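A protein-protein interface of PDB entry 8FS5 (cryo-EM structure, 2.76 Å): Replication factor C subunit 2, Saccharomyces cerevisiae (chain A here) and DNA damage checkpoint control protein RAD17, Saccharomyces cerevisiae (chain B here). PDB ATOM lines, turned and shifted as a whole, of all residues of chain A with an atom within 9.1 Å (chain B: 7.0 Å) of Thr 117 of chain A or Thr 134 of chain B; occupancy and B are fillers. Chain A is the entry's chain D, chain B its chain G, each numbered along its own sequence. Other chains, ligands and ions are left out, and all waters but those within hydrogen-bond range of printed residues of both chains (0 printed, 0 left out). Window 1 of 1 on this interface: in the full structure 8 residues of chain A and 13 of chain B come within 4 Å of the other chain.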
ATOM      1  N   SER A  90     -29.363  12.684  29.747  1.00  0.00           N
ATOM      2  CA  SER A  90     -27.936  12.403  29.714  1.00  0.00           C
ATOM      3  C   SER A  90     -27.111  13.312  30.615  1.00  0.00           C
ATOM      4  O   SER A  90     -26.013  12.917  31.020  1.00  0.00           O
ATOM      5  CB  SER A  90     -27.406  12.514  28.278  1.00  0.00           C
ATOM      6  OG  SER A  90     -27.505  13.843  27.800  1.00  0.00           O
ATOM      7  N   ARG A  91     -27.600  14.510  30.939  1.00  0.00           N
ATOM      8  CA  ARG A  91     -26.820  15.468  31.713  1.00  0.00           C
ATOM      9  C   ARG A  91     -27.298  15.623  33.152  1.00  0.00           C
ATOM     10  O   ARG A  91     -26.854  16.547  33.841  1.00  0.00           O
ATOM     11  CB  ARG A  91     -26.825  16.831  31.018  1.00  0.00           C
ATOM     12  CG  ARG A  91     -26.243  16.814  29.619  1.00  0.00           C
ATOM     13  CD  ARG A  91     -24.754  17.107  29.629  1.00  0.00           C
ATOM     14  NE  ARG A  91     -24.476  18.485  29.246  1.00  0.00           N
ATOM     15  CZ  ARG A  91     -24.274  18.890  28.000  1.00  0.00           C
ATOM     16  NH1 ARG A  91     -24.312  18.044  26.983  1.00  0.00           N
ATOM     17  NH2 ARG A  91     -24.027  20.177  27.768  1.00  0.00           N
ATOM     18  N   LYS A 111     -19.099   9.290  41.828  1.00  0.00           N
ATOM     19  CA  LYS A 111     -17.767   9.583  41.318  1.00  0.00           C
ATOM     20  C   LYS A 111     -17.619   9.258  39.838  1.00  0.00           C
ATOM     21  O   LYS A 111     -17.000  10.035  39.103  1.00  0.00           O
ATOM     22  CB  LYS A 111     -16.715   8.816  42.123  1.00  0.00           C
ATOM     23  CG  LYS A 111     -15.284   9.233  41.833  1.00  0.00           C
ATOM     24  CD  LYS A 111     -14.301   8.458  42.692  1.00  0.00           C
ATOM     25  CE  LYS A 111     -12.870   8.881  42.409  1.00  0.00           C
ATOM     26  NZ  LYS A 111     -11.886   8.021  43.123  1.00  0.00           N
ATOM     27  N   ASN A 112     -18.176   8.134  39.377  1.00  0.00           N
ATOM     28  CA  ASN A 112     -18.112   7.799  37.961  1.00  0.00           C
ATOM     29  C   ASN A 112     -18.975   8.724  37.114  1.00  0.00           C
ATOM     30  O   ASN A 112     -18.590   9.058  35.988  1.00  0.00           O
ATOM     31  CB  ASN A 112     -18.530   6.345  37.741  1.00  0.00           C
ATOM     32  CG  ASN A 112     -17.505   5.360  38.267  1.00  0.00           C
ATOM     33  OD1 ASN A 112     -16.369   5.728  38.567  1.00  0.00           O
ATOM     34  ND2 ASN A 112     -17.902   4.098  38.381  1.00  0.00           N
ATOM     35  N   PHE A 113     -20.137   9.145  37.623  1.00  0.00           N
ATOM     36  CA  PHE A 113     -20.939  10.108  36.878  1.00  0.00           C
ATOM     37  C   PHE A 113     -20.260  11.469  36.808  1.00  0.00           C
ATOM     38  O   PHE A 113     -20.358  12.152  35.782  1.00  0.00           O
ATOM     39  CB  PHE A 113     -22.331  10.246  37.496  1.00  0.00           C
ATOM     40  CG  PHE A 113     -23.281  11.063  36.665  1.00  0.00           C
ATOM     41  CD1 PHE A 113     -24.019  10.472  35.653  1.00  0.00           C
ATOM     42  CD2 PHE A 113     -23.434  12.422  36.890  1.00  0.00           C
ATOM     43  CE1 PHE A 113     -24.891  11.218  34.883  1.00  0.00           C
ATOM     44  CE2 PHE A 113     -24.303  13.174  36.123  1.00  0.00           C
ATOM     45  CZ  PHE A 113     -25.033  12.572  35.118  1.00  0.00           C
ATOM     46  N   ALA A 114     -19.577  11.882  37.878  1.00  0.00           N
ATOM     47  CA  ALA A 114     -18.817  13.127  37.835  1.00  0.00           C
ATOM     48  C   ALA A 114     -17.629  13.013  36.889  1.00  0.00           C
ATOM     49  O   ALA A 114     -17.281  13.980  36.200  1.00  0.00           O
ATOM     50  CB  ALA A 114     -18.355  13.509  39.240  1.00  0.00           C
ATOM     51  N   ARG A 115     -16.994  11.840  36.841  1.00  0.00           N
ATOM     52  CA  ARG A 115     -15.860  11.627  35.949  1.00  0.00           C
ATOM     53  C   ARG A 115     -16.280  11.499  34.491  1.00  0.00           C
ATOM     54  O   ARG A 115     -15.419  11.500  33.604  1.00  0.00           O
ATOM     55  CB  ARG A 115     -15.090  10.376  36.371  1.00  0.00           C
ATOM     56  CG  ARG A 115     -13.730  10.657  36.973  1.00  0.00           C
ATOM     57  CD  ARG A 115     -13.084   9.380  37.499  1.00  0.00           C
ATOM     58  NE  ARG A 115     -12.676   8.445  36.452  1.00  0.00           N
ATOM     59  CZ  ARG A 115     -11.828   8.706  35.463  1.00  0.00           C
ATOM     60  NH1 ARG A 115     -11.203   9.869  35.366  1.00  0.00           N
ATOM     61  NH2 ARG A 115     -11.585   7.764  34.556  1.00  0.00           N
ATOM     62  N   LEU A 116     -17.579  11.380  34.223  1.00  0.00           N
ATOM     63  CA  LEU A 116     -18.050  11.173  32.861  1.00  0.00           C
ATOM     64  C   LEU A 116     -17.793  12.409  32.006  1.00  0.00           C
ATOM     65  O   LEU A 116     -17.693  13.532  32.509  1.00  0.00           O
ATOM     66  CB  LEU A 116     -19.541  10.833  32.860  1.00  0.00           C
ATOM     67  CG  LEU A 116     -19.887   9.365  32.619  1.00  0.00           C
ATOM     68  CD1 LEU A 116     -21.379   9.125  32.790  1.00  0.00           C
ATOM     69  CD2 LEU A 116     -19.427   8.936  31.237  1.00  0.00           C
ATOM     70  N   THR A 117     -17.669  12.187  30.703  1.00  0.00           N
ATOM     71  CA  THR A 117     -17.487  13.265  29.745  1.00  0.00           C
ATOM     72  C   THR A 117     -18.832  13.891  29.400  1.00  0.00           C
ATOM     73  O   THR A 117     -19.851  13.201  29.294  1.00  0.00           O
ATOM     74  CB  THR A 117     -16.805  12.750  28.474  1.00  0.00           C
ATOM     75  OG1 THR A 117     -15.685  11.931  28.831  1.00  0.00           O
ATOM     76  CG2 THR A 117     -16.315  13.908  27.618  1.00  0.00           C
ATOM     77  N   VAL A 118     -18.829  15.212  29.239  1.00  0.00           N
ATOM     78  CA  VAL A 118     -20.038  15.947  28.875  1.00  0.00           C
ATOM     79  C   VAL A 118     -20.459  15.506  27.475  1.00  0.00           C
ATOM     80  O   VAL A 118     -19.669  15.571  26.530  1.00  0.00           O
ATOM     81  CB  VAL A 118     -19.814  17.463  28.941  1.00  0.00           C
ATOM     82  CG1 VAL A 118     -20.872  18.197  28.136  1.00  0.00           C
ATOM     83  CG2 VAL A 118     -19.824  17.932  30.386  1.00  0.00           C
ATOM     84  N   SER A 119     -21.705  15.051  27.345  1.00  0.00           N
ATOM     85  CA  SER A 119     -22.219  14.555  26.074  1.00  0.00           C
ATOM     86  C   SER A 119     -22.374  15.684  25.064  1.00  0.00           C
ATOM     87  O   SER A 119     -22.564  16.844  25.445  1.00  0.00           O
ATOM     88  CB  SER A 119     -23.556  13.842  26.283  1.00  0.00           C
ATOM     89  OG  SER A 119     -24.530  14.729  26.806  1.00  0.00           O
ATOM     90  N   LYS A 120     -22.292  15.353  23.772  1.00  0.00           N
ATOM     91  CA  LYS A 120     -22.437  16.349  22.716  1.00  0.00           C
ATOM     92  C   LYS A 120     -23.884  16.816  22.630  1.00  0.00           C
ATOM     93  O   LYS A 120     -24.784  15.989  22.438  1.00  0.00           O
ATOM     94  CB  LYS A 120     -22.014  15.781  21.368  1.00  0.00           C
ATOM     95  CG  LYS A 120     -20.631  16.202  20.902  1.00  0.00           C
ATOM     96  CD  LYS A 120     -20.103  15.245  19.845  1.00  0.00           C
ATOM     97  CE  LYS A 120     -18.585  15.215  19.827  1.00  0.00           C
ATOM     98  NZ  LYS A 120     -18.046  15.222  18.439  1.00  0.00           N
ATOM     99  N   PRO A 133     -21.732  23.597  29.456  1.00  0.00           N
ATOM    100  CA  PRO A 133     -20.772  22.497  29.291  1.00  0.00           C
ATOM    101  C   PRO A 133     -20.491  21.740  30.580  1.00  0.00           C
ATOM    102  O   PRO A 133     -19.329  21.482  30.910  1.00  0.00           O
ATOM    103  CB  PRO A 133     -19.517  23.217  28.786  1.00  0.00           C
ATOM    104  CG  PRO A 133     -19.599  24.557  29.441  1.00  0.00           C
ATOM    105  CD  PRO A 133     -21.067  24.912  29.448  1.00  0.00           C
ATOM    106  N   TYR A 134     -21.540  21.376  31.313  1.00  0.00           N
ATOM    107  CA  TYR A 134     -21.395  20.589  32.528  1.00  0.00           C
ATOM    108  C   TYR A 134     -22.712  19.885  32.819  1.00  0.00           C
ATOM    109  O   TYR A 134     -23.758  20.218  32.258  1.00  0.00           O
ATOM    110  CB  TYR A 134     -20.961  21.455  33.720  1.00  0.00           C
ATOM    111  CG  TYR A 134     -21.738  22.742  33.887  1.00  0.00           C
ATOM    112  CD1 TYR A 134     -23.008  22.745  34.452  1.00  0.00           C
ATOM    113  CD2 TYR A 134     -21.197  23.958  33.487  1.00  0.00           C
ATOM    114  CE1 TYR A 134     -23.719  23.920  34.607  1.00  0.00           C
ATOM    115  CE2 TYR A 134     -21.901  25.136  33.640  1.00  0.00           C
ATOM    116  CZ  TYR A 134     -23.159  25.112  34.202  1.00  0.00           C
ATOM    117  OH  TYR A 134     -23.862  26.286  34.351  1.00  0.00           O
ATOM    118  N   LYS A 135     -22.646  18.900  33.706  1.00  0.00           N
ATOM    119  CA  LYS A 135     -23.817  18.175  34.174  1.00  0.00           C
ATOM    120  C   LYS A 135     -24.060  18.482  35.645  1.00  0.00           C
ATOM    121  O   LYS A 135     -23.186  18.983  36.357  1.00  0.00           O
ATOM    122  CB  LYS A 135     -23.650  16.668  33.954  1.00  0.00           C
ATOM    123  CG  LYS A 135     -22.218  16.184  34.045  1.00  0.00           C
ATOM    124  CD  LYS A 135     -22.022  14.923  33.227  1.00  0.00           C
ATOM    125  CE  LYS A 135     -20.643  14.339  33.453  1.00  0.00           C
ATOM    126  NZ  LYS A 135     -19.591  15.390  33.473  1.00  0.00           N
ATOM    127  N   TYR A 160     -13.864  17.573  40.059  1.00  0.00           N
ATOM    128  CA  TYR A 160     -14.616  17.572  38.809  1.00  0.00           C
ATOM    129  C   TYR A 160     -15.651  18.693  38.773  1.00  0.00           C
ATOM    130  O   TYR A 160     -16.757  18.525  38.258  1.00  0.00           O
ATOM    131  CB  TYR A 160     -15.284  16.218  38.589  1.00  0.00           C
ATOM    132  CG  TYR A 160     -14.370  15.048  38.871  1.00  0.00           C
ATOM    133  CD1 TYR A 160     -13.283  14.779  38.049  1.00  0.00           C
ATOM    134  CD2 TYR A 160     -14.589  14.219  39.962  1.00  0.00           C
ATOM    135  CE1 TYR A 160     -12.441  13.715  38.305  1.00  0.00           C
ATOM    136  CE2 TYR A 160     -13.753  13.150  40.225  1.00  0.00           C
ATOM    137  CZ  TYR A 160     -12.681  12.904  39.395  1.00  0.00           C
ATOM    138  OH  TYR A 160     -11.845  11.841  39.651  1.00  0.00           O
ATOM    139  N   VAL A 163     -16.551  20.062  35.199  1.00  0.00           N
ATOM    140  CA  VAL A 163     -17.318  19.163  34.342  1.00  0.00           C
ATOM    141  C   VAL A 163     -18.602  18.670  34.988  1.00  0.00           C
ATOM    142  O   VAL A 163     -19.482  18.145  34.282  1.00  0.00           O
ATOM    143  CB  VAL A 163     -16.440  17.966  33.903  1.00  0.00           C
ATOM    144  CG1 VAL A 163     -16.411  16.893  34.981  1.00  0.00           C
ATOM    145  CG2 VAL A 163     -16.910  17.401  32.570  1.00  0.00           C
ATOM    146  N   THR A 164     -18.781  18.817  36.299  1.00  0.00           N
ATOM    147  CA  THR A 164     -19.964  18.327  36.994  1.00  0.00           C
ATOM    148  C   THR A 164     -20.295  19.256  38.152  1.00  0.00           C
ATOM    149  O   THR A 164     -19.418  19.611  38.946  1.00  0.00           O
ATOM    150  CB  THR A 164     -19.744  16.892  37.505  1.00  0.00           C
ATOM    151  OG1 THR A 164     -19.884  15.970  36.416  1.00  0.00           O
ATOM    152  CG2 THR A 164     -20.748  16.538  38.590  1.00  0.00           C
ATOM    153  N   LYS B  81      -7.265  11.111  22.580  1.00  0.00           N
ATOM    154  CA  LYS B  81      -7.198  10.385  23.842  1.00  0.00           C
ATOM    155  C   LYS B  81      -8.600  10.187  24.405  1.00  0.00           C
ATOM    156  O   LYS B  81      -9.393  11.134  24.455  1.00  0.00           O
ATOM    157  CB  LYS B  81      -6.334  11.132  24.859  1.00  0.00           C
ATOM    158  CG  LYS B  81      -4.893  11.339  24.434  1.00  0.00           C
ATOM    159  CD  LYS B  81      -4.223  12.445  25.241  1.00  0.00           C
ATOM    160  CE  LYS B  81      -4.545  12.342  26.723  1.00  0.00           C
ATOM    161  NZ  LYS B  81      -3.888  11.165  27.358  1.00  0.00           N
ATOM    162  N   LEU B  82      -8.900   8.959  24.824  1.00  0.00           N
ATOM    163  CA  LEU B  82     -10.166   8.638  25.468  1.00  0.00           C
ATOM    164  C   LEU B  82      -9.915   7.689  26.629  1.00  0.00           C
ATOM    165  O   LEU B  82      -9.034   6.826  26.558  1.00  0.00           O
ATOM    166  CB  LEU B  82     -11.168   8.004  24.491  1.00  0.00           C
ATOM    167  CG  LEU B  82     -10.714   6.817  23.641  1.00  0.00           C
ATOM    168  CD1 LEU B  82     -11.886   5.891  23.372  1.00  0.00           C
ATOM    169  CD2 LEU B  82     -10.110   7.291  22.334  1.00  0.00           C
ATOM    170  N   CYS B  83     -10.692   7.853  27.695  1.00  0.00           N
ATOM    171  CA  CYS B  83     -10.584   7.030  28.891  1.00  0.00           C
ATOM    172  C   CYS B  83     -11.899   6.300  29.124  1.00  0.00           C
ATOM    173  O   CYS B  83     -12.933   6.934  29.354  1.00  0.00           O
ATOM    174  CB  CYS B  83     -10.223   7.886  30.106  1.00  0.00           C
ATOM    175  SG  CYS B  83     -10.654   7.154  31.697  1.00  0.00           S
ATOM    176  N   VAL B  84     -11.855   4.966  29.061  1.00  0.00           N
ATOM    177  CA  VAL B  84     -13.027   4.126  29.272  1.00  0.00           C
ATOM    178  C   VAL B  84     -12.688   3.066  30.311  1.00  0.00           C
ATOM    179  O   VAL B  84     -11.522   2.785  30.591  1.00  0.00           O
ATOM    180  CB  VAL B  84     -13.524   3.455  27.968  1.00  0.00           C
ATOM    181  CG1 VAL B  84     -13.652   4.474  26.845  1.00  0.00           C
ATOM    182  CG2 VAL B  84     -12.594   2.322  27.560  1.00  0.00           C
ATOM    183  N   LYS B  85     -13.734   2.486  30.895  1.00  0.00           N
ATOM    184  CA  LYS B  85     -13.561   1.432  31.885  1.00  0.00           C
ATOM    185  C   LYS B  85     -13.272   0.099  31.208  1.00  0.00           C
ATOM    186  O   LYS B  85     -13.839  -0.219  30.159  1.00  0.00           O
ATOM    187  CB  LYS B  85     -14.806   1.311  32.763  1.00  0.00           C
ATOM    188  CG  LYS B  85     -15.154   2.573  33.528  1.00  0.00           C
ATOM    189  CD  LYS B  85     -14.039   2.962  34.483  1.00  0.00           C
ATOM    190  CE  LYS B  85     -14.453   4.120  35.375  1.00  0.00           C
ATOM    191  NZ  LYS B  85     -13.317   4.628  36.192  1.00  0.00           N
ATOM    192  N   TYR B 110     -15.054   6.193  16.936  1.00  0.00           N
ATOM    193  CA  TYR B 110     -15.000   7.264  17.925  1.00  0.00           C
ATOM    194  C   TYR B 110     -15.207   8.583  17.197  1.00  0.00           C
ATOM    195  O   TYR B 110     -14.474   8.887  16.251  1.00  0.00           O
ATOM    196  CB  TYR B 110     -13.665   7.260  18.675  1.00  0.00           C
ATOM    197  CG  TYR B 110     -13.630   8.180  19.875  1.00  0.00           C
ATOM    198  CD1 TYR B 110     -14.490   7.985  20.948  1.00  0.00           C
ATOM    199  CD2 TYR B 110     -12.739   9.242  19.936  1.00  0.00           C
ATOM    200  CE1 TYR B 110     -14.461   8.822  22.047  1.00  0.00           C
ATOM    201  CE2 TYR B 110     -12.703  10.085  21.031  1.00  0.00           C
ATOM    202  CZ  TYR B 110     -13.567   9.869  22.083  1.00  0.00           C
ATOM    203  OH  TYR B 110     -13.535  10.705  23.176  1.00  0.00           O
ATOM    204  N   GLY B 112     -15.186  11.697  18.618  1.00  0.00           N
ATOM    205  CA  GLY B 112     -14.584  12.833  19.288  1.00  0.00           C
ATOM    206  C   GLY B 112     -14.944  12.879  20.764  1.00  0.00           C
ATOM    207  O   GLY B 112     -15.634  12.010  21.300  1.00  0.00           O
ATOM    208  N   HIS B 113     -14.448  13.931  21.415  1.00  0.00           N
ATOM    209  CA  HIS B 113     -14.686  14.115  22.840  1.00  0.00           C
ATOM    210  C   HIS B 113     -16.170  14.327  23.115  1.00  0.00           C
ATOM    211  O   HIS B 113     -16.821  15.171  22.494  1.00  0.00           O
ATOM    212  CB  HIS B 113     -13.879  15.305  23.361  1.00  0.00           C
ATOM    213  CG  HIS B 113     -13.599  15.250  24.830  1.00  0.00           C
ATOM    214  ND1 HIS B 113     -12.901  14.218  25.417  1.00  0.00           N
ATOM    215  CD2 HIS B 113     -13.920  16.104  25.830  1.00  0.00           C
ATOM    216  CE1 HIS B 113     -12.806  14.436  26.716  1.00  0.00           C
ATOM    217  NE2 HIS B 113     -13.415  15.575  26.994  1.00  0.00           N
ATOM    218  N   GLY B 114     -16.701  13.559  24.065  1.00  0.00           N
ATOM    219  CA  GLY B 114     -18.111  13.563  24.369  1.00  0.00           C
ATOM    220  C   GLY B 114     -18.908  12.463  23.700  1.00  0.00           C
ATOM    221  O   GLY B 114     -20.030  12.179  24.133  1.00  0.00           O
ATOM    222  N   SER B 115     -18.363  11.842  22.661  1.00  0.00           N
ATOM    223  CA  SER B 115     -18.995  10.726  21.978  1.00  0.00           C
ATOM    224  C   SER B 115     -18.537   9.406  22.583  1.00  0.00           C
ATOM    225  O   SER B 115     -17.411   9.293  23.075  1.00  0.00           O
ATOM    226  CB  SER B 115     -18.658  10.766  20.489  1.00  0.00           C
ATOM    227  OG  SER B 115     -19.138  11.957  19.890  1.00  0.00           O
ATOM    228  N   PRO B 116     -19.388   8.386  22.569  1.00  0.00           N
ATOM    229  CA  PRO B 116     -19.004   7.085  23.118  1.00  0.00           C
ATOM    230  C   PRO B 116     -18.114   6.302  22.158  1.00  0.00           C
ATOM    231  O   PRO B 116     -18.007   6.608  20.969  1.00  0.00           O
ATOM    232  CB  PRO B 116     -20.356   6.384  23.309  1.00  0.00           C
ATOM    233  CG  PRO B 116     -21.201   6.944  22.224  1.00  0.00           C
ATOM    234  CD  PRO B 116     -20.780   8.387  22.082  1.00  0.00           C
ATOM    235  N   PHE B 117     -17.469   5.277  22.708  1.00  0.00           N
ATOM    236  CA  PHE B 117     -16.640   4.369  21.926  1.00  0.00           C
ATOM    237  C   PHE B 117     -17.511   3.219  21.433  1.00  0.00           C
ATOM    238  O   PHE B 117     -18.065   2.464  22.238  1.00  0.00           O
ATOM    239  CB  PHE B 117     -15.472   3.847  22.763  1.00  0.00           C
ATOM    240  CG  PHE B 117     -14.368   3.234  21.950  1.00  0.00           C
ATOM    241  CD1 PHE B 117     -13.759   3.948  20.932  1.00  0.00           C
ATOM    242  CD2 PHE B 117     -13.937   1.942  22.205  1.00  0.00           C
ATOM    243  CE1 PHE B 117     -12.743   3.388  20.184  1.00  0.00           C
ATOM    244  CE2 PHE B 117     -12.922   1.375  21.459  1.00  0.00           C
ATOM    245  CZ  PHE B 117     -12.323   2.099  20.447  1.00  0.00           C
ATOM    246  N   TYR B 132     -19.510   2.494  24.541  1.00  0.00           N
ATOM    247  CA  TYR B 132     -18.884   2.607  25.850  1.00  0.00           C
ATOM    248  C   TYR B 132     -18.740   4.071  26.240  1.00  0.00           C
ATOM    249  O   TYR B 132     -18.258   4.892  25.455  1.00  0.00           O
ATOM    250  CB  TYR B 132     -17.513   1.931  25.855  1.00  0.00           C
ATOM    251  CG  TYR B 132     -17.543   0.474  25.459  1.00  0.00           C
ATOM    252  CD1 TYR B 132     -18.016  -0.495  26.333  1.00  0.00           C
ATOM    253  CD2 TYR B 132     -17.092   0.067  24.210  1.00  0.00           C
ATOM    254  CE1 TYR B 132     -18.043  -1.829  25.973  1.00  0.00           C
ATOM    255  CE2 TYR B 132     -17.114  -1.263  23.842  1.00  0.00           C
ATOM    256  CZ  TYR B 132     -17.590  -2.206  24.726  1.00  0.00           C
ATOM    257  OH  TYR B 132     -17.613  -3.532  24.359  1.00  0.00           O
ATOM    258  N   SER B 133     -19.160   4.391  27.460  1.00  0.00           N
ATOM    259  CA  SER B 133     -19.064   5.752  27.962  1.00  0.00           C
ATOM    260  C   SER B 133     -17.609   6.123  28.223  1.00  0.00           C
ATOM    261  O   SER B 133     -16.849   5.346  28.808  1.00  0.00           O
ATOM    262  CB  SER B 133     -19.883   5.906  29.243  1.00  0.00           C
ATOM    263  OG  SER B 133     -19.847   4.720  30.017  1.00  0.00           O
ATOM    264  N   THR B 134     -17.226   7.317  27.783  1.00  0.00           N
ATOM    265  CA  THR B 134     -15.870   7.821  27.948  1.00  0.00           C
ATOM    266  C   THR B 134     -15.808   8.727  29.169  1.00  0.00           C
ATOM    267  O   THR B 134     -16.689   9.571  29.368  1.00  0.00           O
ATOM    268  CB  THR B 134     -15.408   8.580  26.702  1.00  0.00           C
ATOM    269  OG1 THR B 134     -16.267   9.705  26.480  1.00  0.00           O
ATOM    270  CG2 THR B 134     -15.444   7.671  25.483  1.00  0.00           C
ATOM    271  N   TYR B 135     -14.774   8.548  29.982  1.00  0.00           N
ATOM    272  CA  TYR B 135     -14.600   9.298  31.216  1.00  0.00           C
ATOM    273  C   TYR B 135     -13.442  10.281  31.091  1.00  0.00           C
ATOM    274  O   TYR B 135     -12.630  10.211  30.165  1.00  0.00           O
ATOM    275  CB  TYR B 135     -14.360   8.352  32.396  1.00  0.00           C
ATOM    276  CG  TYR B 135     -15.516   7.418  32.679  1.00  0.00           C
ATOM    277  CD1 TYR B 135     -15.686   6.248  31.949  1.00  0.00           C
ATOM    278  CD2 TYR B 135     -16.437   7.705  33.677  1.00  0.00           C
ATOM    279  CE1 TYR B 135     -16.743   5.396  32.203  1.00  0.00           C
ATOM    280  CE2 TYR B 135     -17.495   6.857  33.939  1.00  0.00           C
ATOM    281  CZ  TYR B 135     -17.643   5.704  33.200  1.00  0.00           C
ATOM    282  OH  TYR B 135     -18.695   4.856  33.457  1.00  0.00           O
ATOM    283  N   LEU B 136     -13.386  11.213  32.040  1.00  0.00           N
ATOM    284  CA  LEU B 136     -12.309  12.193  32.063  1.00  0.00           C
ATOM    285  C   LEU B 136     -10.979  11.514  32.371  1.00  0.00           C
ATOM    286  O   LEU B 136     -10.918  10.500  33.071  1.00  0.00           O
ATOM    287  CB  LEU B 136     -12.600  13.283  33.094  1.00  0.00           C
ATOM    288  CG  LEU B 136     -12.291  14.714  32.653  1.00  0.00           C
ATOM    289  CD1 LEU B 136     -13.261  15.164  31.570  1.00  0.00           C
ATOM    290  CD2 LEU B 136     -12.331  15.663  33.839  1.00  0.00           C
ATOM    291  N   ILE B 137      -9.910  12.085  31.839  1.00  0.00           N
ATOM    292  CA  ILE B 137      -8.578  11.503  31.941  1.00  0.00           C
ATOM    293  C   ILE B 137      -7.884  12.045  33.182  1.00  0.00           C
ATOM    294  O   ILE B 137      -7.911  13.251  33.452  1.00  0.00           O
ATOM    295  CB  ILE B 137      -7.767  11.792  30.665  1.00  0.00           C
ATOM    296  CG1 ILE B 137      -8.491  11.201  29.454  1.00  0.00           C
ATOM    297  CG2 ILE B 137      -6.359  11.228  30.778  1.00  0.00           C
ATOM    298  CD1 ILE B 137      -7.717  11.294  28.174  1.00  0.00           C
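Of the 18 printed residues of chain B, 9 touch a printed residue of chain A.
Printed residues of chain B that touch a printed residue of chain A: Cys 83, Lys 85, His 113, Gly 114, Ser 115, Ser 133, Thr 134, Tyr 135 and Leu 136.
Hydrophobic or aromatic side chains of chain B within 4 Å of the printed part of chain A: His 113, Tyr 135 and Leu 136.
Hydrophobic or aromatic side chains of chain A that line the printed part of chain B: Leu 116.
The side-chain sulfur (SG) of Cys 83 of chain B is in hydrogen-bond range of the guanidinium group (NH2) of Arg 115 of chain A.
O of Arg 115 of chain A sits at hydrogen-bond distance from N of Leu 136 of chain B (2.6 Å).
The backbone carbonyl oxygen (O) of Thr 134 of chain B sits at hydrogen-bond distance from the side-chain hydroxyl (OG1) of Thr 117 of chain A (2.6 Å).
Phe 113 of chain A touches none of the printed residues of chain B.
Printed residues of chain B within 4 Å of Arg 115 of chain A: Cys 83 (3.1 Å), Lys 85 (3.9 Å), Tyr 135 (3.3 Å) and Leu 136 (2.4 Å).
Of the printed residues of chain B, Thr 117 of chain A touches His 113, Gly 114, Thr 134 and Tyr 135.
Of the printed residues of chain A, His 113 of chain B touches Thr 117 and Lys 120.
Of chain A, only Leu 116 and Thr 117 come within 4 Å of Thr 134 of chain B.
The nearest printed residue of chain B that does not touch Thr 117 of chain A is Leu 136 of chain B (4.01 Å).
The nearest residue of chain A that does not touch Thr 134 of chain B is Arg 115 of chain A (4.8 Å).
The nearest printed residue of chain A that does not touch Tyr 135 of chain B is Phe 113 of chain A (5.1 Å).
O of Asn 112 of chain A touches CE2 of Tyr 135 of chain B, 3.2 Å away.
NE of Arg 115 of chain A touches NZ of Lys 85 of chain B, at 3.9 Å.
Tyr 135 of chain B touches Arg 115 of chain A (CA to O, 3.3 Å).
CD2 of Leu 116 of chain A touches CB of Ser 133 of chain B, at 3.7 Å.
Leu 116 of chain A touches Thr 134 of chain B.
CG of Leu 116 of chain A touches CE2 of Tyr 135 of chain B (3.7 Å).
N of Gly 114 of chain B touches CG2 of Thr 117 of chain A, at 3.6 Å.
Gly 114 of chain B touches Val 118 of chain A.
CA of Ser 119 of chain A touches O of Gly 114 of chain B, at 3.8 Å.
His 113 of chain B touches Lys 120 of chain A (O to CE, 3.2 Å).
OG of Ser 90 of chain A lies within hydrogen-bond range of OG of Ser 119 of chain A, 3.3 Å away.
O of Leu 116 of chain A is in hydrogen-bond range of NZ of Lys 135 of chain A (2.8 Å).
SG of Cys 83 of chain B is in hydrogen-bond range of O of Leu 136 of chain B, 3.6 Å away.
O of Ser 119 of chain A sits at hydrogen-bond distance from NH1 of Arg 91 of chain A, at 2.6 Å.
N of Tyr 135 of chain B is in hydrogen-bond range of O of Cys 83 of chain B (2.5 Å).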
